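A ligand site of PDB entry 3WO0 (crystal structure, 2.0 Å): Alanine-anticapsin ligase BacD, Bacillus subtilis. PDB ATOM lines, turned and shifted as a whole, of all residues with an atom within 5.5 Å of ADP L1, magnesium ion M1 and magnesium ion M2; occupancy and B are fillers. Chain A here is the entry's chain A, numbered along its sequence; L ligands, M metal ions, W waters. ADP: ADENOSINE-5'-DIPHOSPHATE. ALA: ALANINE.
Residues that only touch magnesium ion M2: Lys 140 (3.7 Å). Along chain A the residues within 4 Å of magnesium ion M2 span positions 140 to 326. The nearest printed residue that does not touch magnesium ion M2 is Ala 185 (4.4 Å).
The backbone carbonyl oxygen of Phe 273 is in hydrogen-bond range of the side-chain hydroxyl of Ser 187, 2.9 Å away. OE1 of Glu 326 lies close to NZ of Lys 140 (3.2 Å). The backbone NH (N) of Ile 325 is in hydrogen-bond range of the backbone carbonyl oxygen (O) of Glu 313, 2.9 Å away. The backbone carbonyl oxygen (O) of Leu 231 lies within hydrogen-bond range of the side-chain amino group (NZ) of Lys 315, 2.7 Å away. The backbone carbonyl oxygen (O) of Glu 228 is in hydrogen-bond range of the backbone NH (N) of Ile 178, 2.7 Å away. OE2 of Glu 228 lies within salt-bridge range of NE of Arg 144 (2.8 Å). The side-chain amino group (NZ) of Lys 180 lies within salt-bridge range of the side-chain carboxylate (OE1) of Glu 228 (2.8 Å). The backbone carbonyl oxygen (O) of Ile 325 is in hydrogen-bond range of the guanidinium group (NH2) of Arg 144 (3.4 Å).
O of Ala 185 sits close to O1B of ADP L1 (3.4 Å). Merely in contact with ADP L1: Phe 273, Phe 230, Val 190, Ile 325, Ile 178, Ile 188 and Leu 184. Hydrophobic or aromatic side chains that line ADP L1: Ile 178, Val 190, Phe 230, Leu 231, Phe 273 and Ile 325. Within 4 Å of ADP L1: Lys 140, Ile 178, Lys 180, Leu 184, Ala 185, Ser 186, Ser 187, Ile 188, Val 190, Glu 228, Glu 229, Phe 230, Leu 231, Gln 270, Phe 273, Glu 313, Ile 325 and Glu 326.
Magnesium ion M1 is bound by the side-chain carboxylate (OE2) of Glu 326 (1.9 Å), an oxygen (O1A) of ADP L1 (2.0 Å), water W1 (2.0 Å), the side-chain carboxylate (OE1) of Glu 313 (2.2 Å), water W4 (2.3 Å) and an oxygen (O3B) of ADP L1 (2.3 Å).
Water W4 lies within hydrogen-bond range of the side-chain carboxylate (OE2) of Glu 313 (2.5 Å) and an oxygen (O3') of ADP L1 (2.9 Å). Water W2 lies within hydrogen-bond range of the backbone carbonyl oxygen (O) of Leu 184 (2.5 Å) and the side-chain carboxylate (OE1) of Glu 111 (3.1 Å). Water W5 lies within hydrogen-bond range of N3 of ADP L1 and NZ of Lys 315.
Within 4 Å of magnesium ion M1: Glu 313 and Glu 326. The nearest printed residue that does not touch magnesium ion M1 is Ile 325 (5.4 Å).
An oxygen (O2A) of ADP L1 is in salt-bridge range of the side-chain amino group (NZ) of Lys 180. The side-chain amino group of Lys 140 is in hydrogen-bond range of an oxygen (O3A) of ADP L1, 3.5 Å away. The backbone NH of Ser 187 is in hydrogen-bond range of an oxygen (O1B) of ADP L1 (2.5 Å). NE2 of Gln 270 lies within hydrogen-bond range of O2' of ADP L1. OE1 of Glu 228 lies within hydrogen-bond range of N6 of ADP L1 (2.6 Å). N1 of ADP L1 sits at hydrogen-bond distance from N of Leu 231, at 2.8 Å. The side-chain carboxylate of Glu 313 lies within salt-bridge range of a nitrogen (N) of ALA L2 (3.0 Å). The guanidinium group of Arg 330 is in salt-bridge range of an oxygen (O) of ALA L2 (2.8 Å). The side-chain carboxylate (OE1) of Glu 275 lies within salt-bridge range of a nitrogen (N) of ALA L2 (3.0 Å). The backbone NH (N) of Ser 186 is in hydrogen-bond range of an oxygen (O1B) of ADP L1. A nitrogen (N6) of ADP L1 lies within hydrogen-bond range of the backbone carbonyl oxygen of Glu 229 (3.3 Å).
Water W7 is bound to magnesium ion M2, at 1.9 Å. O2B of ADP L1 is bound to magnesium ion M2 (1.9 Å). Magnesium ion M2 is bound by OE2 of Glu 326, 2.0 Å away. Magnesium ion M2 is bound by water W3, at 2.0 Å. OE1 of Glu 326 is bound to magnesium ion M2, at 2.3 Å. Water W2 is bound to magnesium ion M2 (2.3 Å).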
ATOM      1  N   GLU A 111      -7.876  19.802   5.476  1.00  0.00           N
ATOM      2  CA  GLU A 111      -7.638  19.541   4.038  1.00  0.00           C
ATOM      3  C   GLU A 111      -8.617  20.322   3.169  1.00  0.00           C
ATOM      4  O   GLU A 111      -8.233  21.003   2.227  1.00  0.00           O
ATOM      5  CB  GLU A 111      -7.823  18.042   3.732  1.00  0.00           C
ATOM      6  CG  GLU A 111      -6.629  17.138   3.967  1.00  0.00           C
ATOM      7  CD  GLU A 111      -5.447  17.466   3.056  1.00  0.00           C
ATOM      8  OE1 GLU A 111      -5.349  16.900   1.943  1.00  0.00           O
ATOM      9  OE2 GLU A 111      -4.640  18.334   3.434  1.00  0.00           O
ATOM     10  N   LYS A 140      -4.439  15.023  -6.160  1.00  0.00           N
ATOM     11  CA  LYS A 140      -3.298  14.093  -6.155  1.00  0.00           C
ATOM     12  C   LYS A 140      -2.695  13.888  -7.519  1.00  0.00           C
ATOM     13  O   LYS A 140      -1.501  13.613  -7.616  1.00  0.00           O
ATOM     14  CB  LYS A 140      -3.668  12.749  -5.507  1.00  0.00           C
ATOM     15  CG  LYS A 140      -3.835  12.823  -4.000  1.00  0.00           C
ATOM     16  CD  LYS A 140      -4.223  11.477  -3.384  1.00  0.00           C
ATOM     17  CE  LYS A 140      -3.803  11.349  -1.917  1.00  0.00           C
ATOM     18  NZ  LYS A 140      -4.822  11.812  -0.929  1.00  0.00           N
ATOM     19  N   ARG A 144       1.184  14.599  -7.733  1.00  0.00           N
ATOM     20  CA  ARG A 144       2.124  13.667  -8.347  1.00  0.00           C
ATOM     21  C   ARG A 144       2.818  14.225  -9.588  1.00  0.00           C
ATOM     22  O   ARG A 144       4.004  13.977  -9.784  1.00  0.00           O
ATOM     23  CB  ARG A 144       1.444  12.324  -8.672  1.00  0.00           C
ATOM     24  CG  ARG A 144       2.368  11.321  -9.389  1.00  0.00           C
ATOM     25  CD  ARG A 144       3.458  10.803  -8.467  1.00  0.00           C
ATOM     26  NE  ARG A 144       2.875  10.046  -7.373  1.00  0.00           N
ATOM     27  CZ  ARG A 144       3.424   9.918  -6.168  1.00  0.00           C
ATOM     28  NH1 ARG A 144       4.600  10.456  -5.910  1.00  0.00           N
ATOM     29  NH2 ARG A 144       2.805   9.217  -5.235  1.00  0.00           N
ATOM     30  N   ILE A 178      -1.088   1.042  -7.265  1.00  0.00           N
ATOM     31  CA  ILE A 178      -1.915   1.754  -6.282  1.00  0.00           C
ATOM     32  C   ILE A 178      -3.019   2.551  -6.958  1.00  0.00           C
ATOM     33  O   ILE A 178      -2.768   3.425  -7.798  1.00  0.00           O
ATOM     34  CB  ILE A 178      -1.047   2.712  -5.427  1.00  0.00           C
ATOM     35  CG1 ILE A 178      -0.404   1.936  -4.282  1.00  0.00           C
ATOM     36  CG2 ILE A 178      -1.855   3.887  -4.907  1.00  0.00           C
ATOM     37  CD1 ILE A 178      -1.356   1.440  -3.208  1.00  0.00           C
ATOM     38  N   LYS A 180      -6.208   5.004  -5.831  1.00  0.00           N
ATOM     39  CA  LYS A 180      -6.757   5.757  -4.705  1.00  0.00           C
ATOM     40  C   LYS A 180      -7.528   6.996  -5.174  1.00  0.00           C
ATOM     41  O   LYS A 180      -7.248   7.565  -6.249  1.00  0.00           O
ATOM     42  CB  LYS A 180      -5.621   6.145  -3.724  1.00  0.00           C
ATOM     43  CG  LYS A 180      -4.545   7.037  -4.345  1.00  0.00           C
ATOM     44  CD  LYS A 180      -3.273   7.105  -3.471  1.00  0.00           C
ATOM     45  CE  LYS A 180      -2.282   8.079  -4.101  1.00  0.00           C
ATOM     46  NZ  LYS A 180      -1.052   8.263  -3.274  1.00  0.00           N
ATOM     47  N   LEU A 184      -9.524  12.842  -1.074  1.00  0.00           N
ATOM     48  CA  LEU A 184      -9.914  12.497   0.294  1.00  0.00           C
ATOM     49  C   LEU A 184      -8.673  12.375   1.161  1.00  0.00           C
ATOM     50  O   LEU A 184      -7.700  13.103   0.970  1.00  0.00           O
ATOM     51  CB  LEU A 184     -10.733  11.209   0.333  1.00  0.00           C
ATOM     52  CG  LEU A 184     -12.044  11.244  -0.470  1.00  0.00           C
ATOM     53  CD1 LEU A 184     -12.804   9.954  -0.240  1.00  0.00           C
ATOM     54  CD2 LEU A 184     -12.890  12.450  -0.087  1.00  0.00           C
ATOM     55  N   ALA A 185      -8.735  11.512   2.157  1.00  0.00           N
ATOM     56  CA  ALA A 185      -7.690  11.449   3.163  1.00  0.00           C
ATOM     57  C   ALA A 185      -7.895  10.181   3.993  1.00  0.00           C
ATOM     58  O   ALA A 185      -8.794   9.376   3.707  1.00  0.00           O
ATOM     59  CB  ALA A 185      -7.728  12.686   4.052  1.00  0.00           C
ATOM     60  N   SER A 186      -7.020   9.983   4.969  1.00  0.00           N
ATOM     61  CA  SER A 186      -7.173   8.903   5.908  1.00  0.00           C
ATOM     62  C   SER A 186      -7.164   7.540   5.223  1.00  0.00           C
ATOM     63  O   SER A 186      -7.644   6.563   5.794  1.00  0.00           O
ATOM     64  CB  SER A 186      -8.477   9.066   6.698  1.00  0.00           C
ATOM     65  OG  SER A 186      -8.431  10.249   7.455  1.00  0.00           O
ATOM     66  N   SER A 187      -6.557   7.484   4.027  1.00  0.00           N
ATOM     67  CA  SER A 187      -6.425   6.229   3.270  1.00  0.00           C
ATOM     68  C   SER A 187      -7.778   5.751   2.752  1.00  0.00           C
ATOM     69  O   SER A 187      -7.935   4.581   2.379  1.00  0.00           O
ATOM     70  CB  SER A 187      -5.794   5.122   4.116  1.00  0.00           C
ATOM     71  OG  SER A 187      -4.572   5.555   4.671  1.00  0.00           O
ATOM     72  N   ILE A 188      -8.760   6.649   2.710  1.00  0.00           N
ATOM     73  CA  ILE A 188     -10.093   6.278   2.214  1.00  0.00           C
ATOM     74  C   ILE A 188      -9.963   5.889   0.757  1.00  0.00           C
ATOM     75  O   ILE A 188      -9.474   6.665  -0.038  1.00  0.00           O
ATOM     76  CB  ILE A 188     -11.096   7.447   2.393  1.00  0.00           C
ATOM     77  CG1 ILE A 188     -11.279   7.791   3.896  1.00  0.00           C
ATOM     78  CG2 ILE A 188     -12.449   7.107   1.746  1.00  0.00           C
ATOM     79  CD1 ILE A 188     -11.664   9.229   4.190  1.00  0.00           C
ATOM     80  N   VAL A 190      -7.946   3.806  -0.726  1.00  0.00           N
ATOM     81  CA  VAL A 190      -6.615   3.481  -1.257  1.00  0.00           C
ATOM     82  C   VAL A 190      -6.491   1.960  -1.362  1.00  0.00           C
ATOM     83  O   VAL A 190      -6.607   1.242  -0.365  1.00  0.00           O
ATOM     84  CB  VAL A 190      -5.439   4.073  -0.391  1.00  0.00           C
ATOM     85  CG1 VAL A 190      -4.108   3.723  -1.022  1.00  0.00           C
ATOM     86  CG2 VAL A 190      -5.543   5.591  -0.275  1.00  0.00           C
ATOM     87  N   GLU A 228      -1.204   4.678  -9.736  1.00  0.00           N
ATOM     88  CA  GLU A 228       0.204   4.963  -9.759  1.00  0.00           C
ATOM     89  C   GLU A 228       1.012   3.758  -9.275  1.00  0.00           C
ATOM     90  O   GLU A 228       0.488   2.842  -8.586  1.00  0.00           O
ATOM     91  CB  GLU A 228       0.512   6.176  -8.889  1.00  0.00           C
ATOM     92  CG  GLU A 228       0.329   5.902  -7.397  1.00  0.00           C
ATOM     93  CD  GLU A 228       0.550   7.153  -6.543  1.00  0.00           C
ATOM     94  OE1 GLU A 228       0.445   7.024  -5.321  1.00  0.00           O
ATOM     95  OE2 GLU A 228       0.803   8.251  -7.078  1.00  0.00           O
ATOM     96  N   GLU A 229       2.282   3.774  -9.649  1.00  0.00           N
ATOM     97  CA  GLU A 229       3.200   2.717  -9.236  1.00  0.00           C
ATOM     98  C   GLU A 229       3.143   2.604  -7.740  1.00  0.00           C
ATOM     99  O   GLU A 229       3.223   3.607  -7.059  1.00  0.00           O
ATOM    100  CB  GLU A 229       4.633   3.076  -9.630  1.00  0.00           C
ATOM    101  CG  GLU A 229       4.876   3.067 -11.127  1.00  0.00           C
ATOM    102  CD  GLU A 229       6.352   3.183 -11.471  1.00  0.00           C
ATOM    103  OE1 GLU A 229       7.163   2.425 -10.899  1.00  0.00           O
ATOM    104  OE2 GLU A 229       6.690   4.061 -12.300  1.00  0.00           O
ATOM    105  N   PHE A 230       2.971   1.382  -7.229  1.00  0.00           N
ATOM    106  CA  PHE A 230       3.180   1.117  -5.802  1.00  0.00           C
ATOM    107  C   PHE A 230       4.628   1.331  -5.421  1.00  0.00           C
ATOM    108  O   PHE A 230       5.504   0.683  -5.975  1.00  0.00           O
ATOM    109  CB  PHE A 230       2.769  -0.307  -5.440  1.00  0.00           C
ATOM    110  CG  PHE A 230       3.060  -0.676  -4.004  1.00  0.00           C
ATOM    111  CD1 PHE A 230       2.333  -0.126  -2.961  1.00  0.00           C
ATOM    112  CD2 PHE A 230       4.077  -1.584  -3.692  1.00  0.00           C
ATOM    113  CE1 PHE A 230       2.611  -0.455  -1.650  1.00  0.00           C
ATOM    114  CE2 PHE A 230       4.360  -1.909  -2.368  1.00  0.00           C
ATOM    115  CZ  PHE A 230       3.609  -1.360  -1.348  1.00  0.00           C
ATOM    116  N   LEU A 231       4.904   2.269  -4.514  1.00  0.00           N
ATOM    117  CA  LEU A 231       6.264   2.526  -4.082  1.00  0.00           C
ATOM    118  C   LEU A 231       6.706   1.427  -3.098  1.00  0.00           C
ATOM    119  O   LEU A 231       6.131   1.271  -2.021  1.00  0.00           O
ATOM    120  CB  LEU A 231       6.398   3.905  -3.437  1.00  0.00           C
ATOM    121  CG  LEU A 231       5.901   5.127  -4.213  1.00  0.00           C
ATOM    122  CD1 LEU A 231       5.799   6.329  -3.310  1.00  0.00           C
ATOM    123  CD2 LEU A 231       6.824   5.452  -5.386  1.00  0.00           C
ATOM    124  N   TYR A 247       7.717   3.593   5.947  1.00  0.00           N
ATOM    125  CA  TYR A 247       7.344   4.966   5.618  1.00  0.00           C
ATOM    126  C   TYR A 247       7.523   5.800   6.849  1.00  0.00           C
ATOM    127  O   TYR A 247       7.621   5.271   7.961  1.00  0.00           O
ATOM    128  CB  TYR A 247       5.891   5.058   5.063  1.00  0.00           C
ATOM    129  CG  TYR A 247       4.822   5.091   6.119  1.00  0.00           C
ATOM    130  CD1 TYR A 247       4.097   6.283   6.408  1.00  0.00           C
ATOM    131  CD2 TYR A 247       4.441   3.963   6.793  1.00  0.00           C
ATOM    132  CE1 TYR A 247       3.083   6.327   7.366  1.00  0.00           C
ATOM    133  CE2 TYR A 247       3.444   3.995   7.774  1.00  0.00           C
ATOM    134  CZ  TYR A 247       2.715   5.160   7.996  1.00  0.00           C
ATOM    135  OH  TYR A 247       1.752   5.150   8.987  1.00  0.00           O
ATOM    136  N   GLN A 270       1.315  -0.274   9.487  1.00  0.00           N
ATOM    137  CA  GLN A 270      -0.112  -0.052   9.261  1.00  0.00           C
ATOM    138  C   GLN A 270      -0.921  -1.347   9.306  1.00  0.00           C
ATOM    139  O   GLN A 270      -0.356  -2.412   9.225  1.00  0.00           O
ATOM    140  CB  GLN A 270      -0.308   0.593   7.901  1.00  0.00           C
ATOM    141  CG  GLN A 270       0.182   2.000   7.822  1.00  0.00           C
ATOM    142  CD  GLN A 270       0.510   2.423   6.402  1.00  0.00           C
ATOM    143  OE1 GLN A 270       1.460   1.916   5.780  1.00  0.00           O
ATOM    144  NE2 GLN A 270      -0.231   3.406   5.898  1.00  0.00           N
ATOM    145  N   PHE A 273      -3.854  -0.097   5.048  1.00  0.00           N
ATOM    146  CA  PHE A 273      -3.283   1.217   4.851  1.00  0.00           C
ATOM    147  C   PHE A 273      -3.699   2.138   6.007  1.00  0.00           C
ATOM    148  O   PHE A 273      -3.390   3.297   6.007  1.00  0.00           O
ATOM    149  CB  PHE A 273      -3.699   1.763   3.488  1.00  0.00           C
ATOM    150  CG  PHE A 273      -3.054   1.048   2.329  1.00  0.00           C
ATOM    151  CD1 PHE A 273      -1.666   0.998   2.219  1.00  0.00           C
ATOM    152  CD2 PHE A 273      -3.825   0.380   1.391  1.00  0.00           C
ATOM    153  CE1 PHE A 273      -1.054   0.313   1.176  1.00  0.00           C
ATOM    154  CE2 PHE A 273      -3.216  -0.327   0.349  1.00  0.00           C
ATOM    155  CZ  PHE A 273      -1.830  -0.354   0.246  1.00  0.00           C
ATOM    156  N   GLU A 275      -3.264   3.806   9.510  1.00  0.00           N
ATOM    157  CA  GLU A 275      -2.090   4.122  10.372  1.00  0.00           C
ATOM    158  C   GLU A 275      -2.329   3.680  11.796  1.00  0.00           C
ATOM    159  O   GLU A 275      -3.470   3.749  12.298  1.00  0.00           O
ATOM    160  CB  GLU A 275      -1.779   5.606  10.314  1.00  0.00           C
ATOM    161  CG  GLU A 275      -1.474   6.106   8.930  1.00  0.00           C
ATOM    162  CD  GLU A 275      -0.711   7.405   8.951  1.00  0.00           C
ATOM    163  OE1 GLU A 275      -1.373   8.456   8.857  1.00  0.00           O
ATOM    164  OE2 GLU A 275       0.546   7.402   9.118  1.00  0.00           O
ATOM    165  N   GLU A 313       4.515  12.692   3.592  1.00  0.00           N
ATOM    166  CA  GLU A 313       4.667  11.274   3.831  1.00  0.00           C
ATOM    167  C   GLU A 313       5.544  10.651   2.728  1.00  0.00           C
ATOM    168  O   GLU A 313       5.372  10.933   1.547  1.00  0.00           O
ATOM    169  CB  GLU A 313       3.309  10.600   3.902  1.00  0.00           C
ATOM    170  CG  GLU A 313       2.494  10.965   5.146  1.00  0.00           C
ATOM    171  CD  GLU A 313       1.087  10.425   5.074  1.00  0.00           C
ATOM    172  OE1 GLU A 313       0.390  10.760   4.086  1.00  0.00           O
ATOM    173  OE2 GLU A 313       0.695   9.680   5.984  1.00  0.00           O
ATOM    174  N   LYS A 315       7.857   7.150   1.379  1.00  0.00           N
ATOM    175  CA  LYS A 315       8.190   5.709   1.433  1.00  0.00           C
ATOM    176  C   LYS A 315       9.713   5.530   1.431  1.00  0.00           C
ATOM    177  O   LYS A 315      10.445   6.160   0.657  1.00  0.00           O
ATOM    178  CB  LYS A 315       7.589   4.948   0.242  1.00  0.00           C
ATOM    179  CG  LYS A 315       7.452   3.447   0.486  1.00  0.00           C
ATOM    180  CD  LYS A 315       6.291   3.208   1.432  1.00  0.00           C
ATOM    181  CE  LYS A 315       6.123   1.751   1.801  1.00  0.00           C
ATOM    182  NZ  LYS A 315       5.706   0.900   0.662  1.00  0.00           N
ATOM    183  N   ILE A 325       4.980   9.946  -1.122  1.00  0.00           N
ATOM    184  CA  ILE A 325       3.641   9.382  -1.099  1.00  0.00           C
ATOM    185  C   ILE A 325       2.614  10.484  -1.301  1.00  0.00           C
ATOM    186  O   ILE A 325       1.779  10.395  -2.236  1.00  0.00           O
ATOM    187  CB  ILE A 325       3.354   8.655   0.206  1.00  0.00           C
ATOM    188  CG1 ILE A 325       4.374   7.523   0.420  1.00  0.00           C
ATOM    189  CG2 ILE A 325       1.949   8.093   0.217  1.00  0.00           C
ATOM    190  CD1 ILE A 325       4.173   6.780   1.705  1.00  0.00           C
ATOM    191  N   GLU A 326       2.722  11.535  -0.497  1.00  0.00           N
ATOM    192  CA  GLU A 326       1.902  12.740  -0.624  1.00  0.00           C
ATOM    193  C   GLU A 326       2.405  13.826   0.353  1.00  0.00           C
ATOM    194  O   GLU A 326       3.278  13.590   1.219  1.00  0.00           O
ATOM    195  CB  GLU A 326       0.414  12.441  -0.402  1.00  0.00           C
ATOM    196  CG  GLU A 326       0.075  12.102   1.026  1.00  0.00           C
ATOM    197  CD  GLU A 326      -1.372  12.286   1.397  1.00  0.00           C
ATOM    198  OE1 GLU A 326      -2.186  12.849   0.594  1.00  0.00           O
ATOM    199  OE2 GLU A 326      -1.707  11.831   2.522  1.00  0.00           O
ATOM    200  N   ARG A 330      -0.926  21.475   5.476  1.00  0.00           N
ATOM    201  CA  ARG A 330      -1.404  21.676   6.827  1.00  0.00           C
ATOM    202  C   ARG A 330      -0.674  20.753   7.762  1.00  0.00           C
ATOM    203  O   ARG A 330       0.219  19.992   7.331  1.00  0.00           O
ATOM    204  CB  ARG A 330      -2.873  21.398   6.897  1.00  0.00           C
ATOM    205  CG  ARG A 330      -3.289  20.147   6.156  1.00  0.00           C
ATOM    206  CD  ARG A 330      -3.451  18.973   7.066  1.00  0.00           C
ATOM    207  NE  ARG A 330      -3.792  17.767   6.303  1.00  0.00           N
ATOM    208  CZ  ARG A 330      -3.518  16.540   6.722  1.00  0.00           C
ATOM    209  NH1 ARG A 330      -2.954  16.350   7.919  1.00  0.00           N
ATOM    210  NH2 ARG A 330      -3.815  15.513   5.951  1.00  0.00           N
HETATM  211  PB  ADP L   1      -4.519   9.690   2.121  1.00  0.00           P
HETATM  212  O1B ADP L   1      -5.802   8.911   2.072  1.00  0.00           O
HETATM  213  O2B ADP L   1      -4.559  11.156   1.787  1.00  0.00           O
HETATM  214  O3B ADP L   1      -3.836   9.388   3.473  1.00  0.00           O
HETATM  215  PA  ADP L   1      -2.124   8.619   0.873  1.00  0.00           P
HETATM  216  O1A ADP L   1      -1.388   9.045   2.115  1.00  0.00           O
HETATM  217  O2A ADP L   1      -1.585   8.933  -0.514  1.00  0.00           O
HETATM  218  O3A ADP L   1      -3.690   9.087   0.887  1.00  0.00           O
HETATM  219  O5' ADP L   1      -2.321   7.029   0.946  1.00  0.00           O
HETATM  220  C5' ADP L   1      -2.622   6.389   2.189  1.00  0.00           C
HETATM  221  C4' ADP L   1      -1.537   5.356   2.483  1.00  0.00           C
HETATM  222  O4' ADP L   1      -1.536   4.350   1.447  1.00  0.00           O
HETATM  223  C3' ADP L   1      -0.121   5.936   2.533  1.00  0.00           C
HETATM  224  O3' ADP L   1       0.281   6.357   3.837  1.00  0.00           O
HETATM  225  C2' ADP L   1       0.686   4.754   2.070  1.00  0.00           C
HETATM  226  O2' ADP L   1       0.853   3.826   3.127  1.00  0.00           O
HETATM  227  C1' ADP L   1      -0.205   4.059   1.060  1.00  0.00           C
HETATM  228  N9  ADP L   1       0.070   4.552  -0.283  1.00  0.00           N
HETATM  229  C8  ADP L   1      -0.617   5.472  -0.967  1.00  0.00           C
HETATM  230  N7  ADP L   1      -0.040   5.684  -2.164  1.00  0.00           N
HETATM  231  C5  ADP L   1       1.031   4.881  -2.256  1.00  0.00           C
HETATM  232  C6  ADP L   1       2.069   4.587  -3.264  1.00  0.00           C
HETATM  233  N6  ADP L   1       2.061   5.213  -4.465  1.00  0.00           N
HETATM  234  N1  ADP L   1       3.020   3.686  -2.943  1.00  0.00           N
HETATM  235  C2  ADP L   1       3.010   3.041  -1.761  1.00  0.00           C
HETATM  236  N3  ADP L   1       2.101   3.258  -0.812  1.00  0.00           N
HETATM  237  C4  ADP L   1       1.106   4.159  -0.997  1.00  0.00           C
HETATM  238  N   ALA L   2      -1.180  11.215   7.809  1.00  0.00           N
HETATM  239  CA  ALA L   2      -2.253  11.555   8.783  1.00  0.00           C
HETATM  240  C   ALA L   2      -2.678  12.973   8.432  1.00  0.00           C
HETATM  241  O   ALA L   2      -2.536  13.401   7.265  1.00  0.00           O
HETATM  242  CB  ALA L   2      -1.742  11.507  10.220  1.00  0.00           C
HETATM  243  OXT ALA L   2      -3.085  13.688   9.342  1.00  0.00           O
HETATM  244 MG    MG M   1      -1.674  10.291   3.599  1.00  0.00          MG
HETATM  245 MG    MG M   2      -3.568  12.665   2.429  1.00  0.00          MG
HETATM  246  O   HOH W   1      -2.372  11.221   5.252  1.00  0.00           O
HETATM  247  O   HOH W   2      -5.521  13.833   1.887  1.00  0.00           O
HETATM  248  O   HOH W   3      -2.905  14.511   3.008  1.00  0.00           O
HETATM  249  O   HOH W   4      -1.286   8.474   4.998  1.00  0.00           O
HETATM  250  O   HOH W   5       2.886   1.682   1.250  1.00  0.00           O
HETATM  251  O   HOH W   6      -3.991   7.965   5.564  1.00  0.00           O
HETATM  252  O   HOH W   7      -4.166  12.510   4.223  1.00  0.00           O
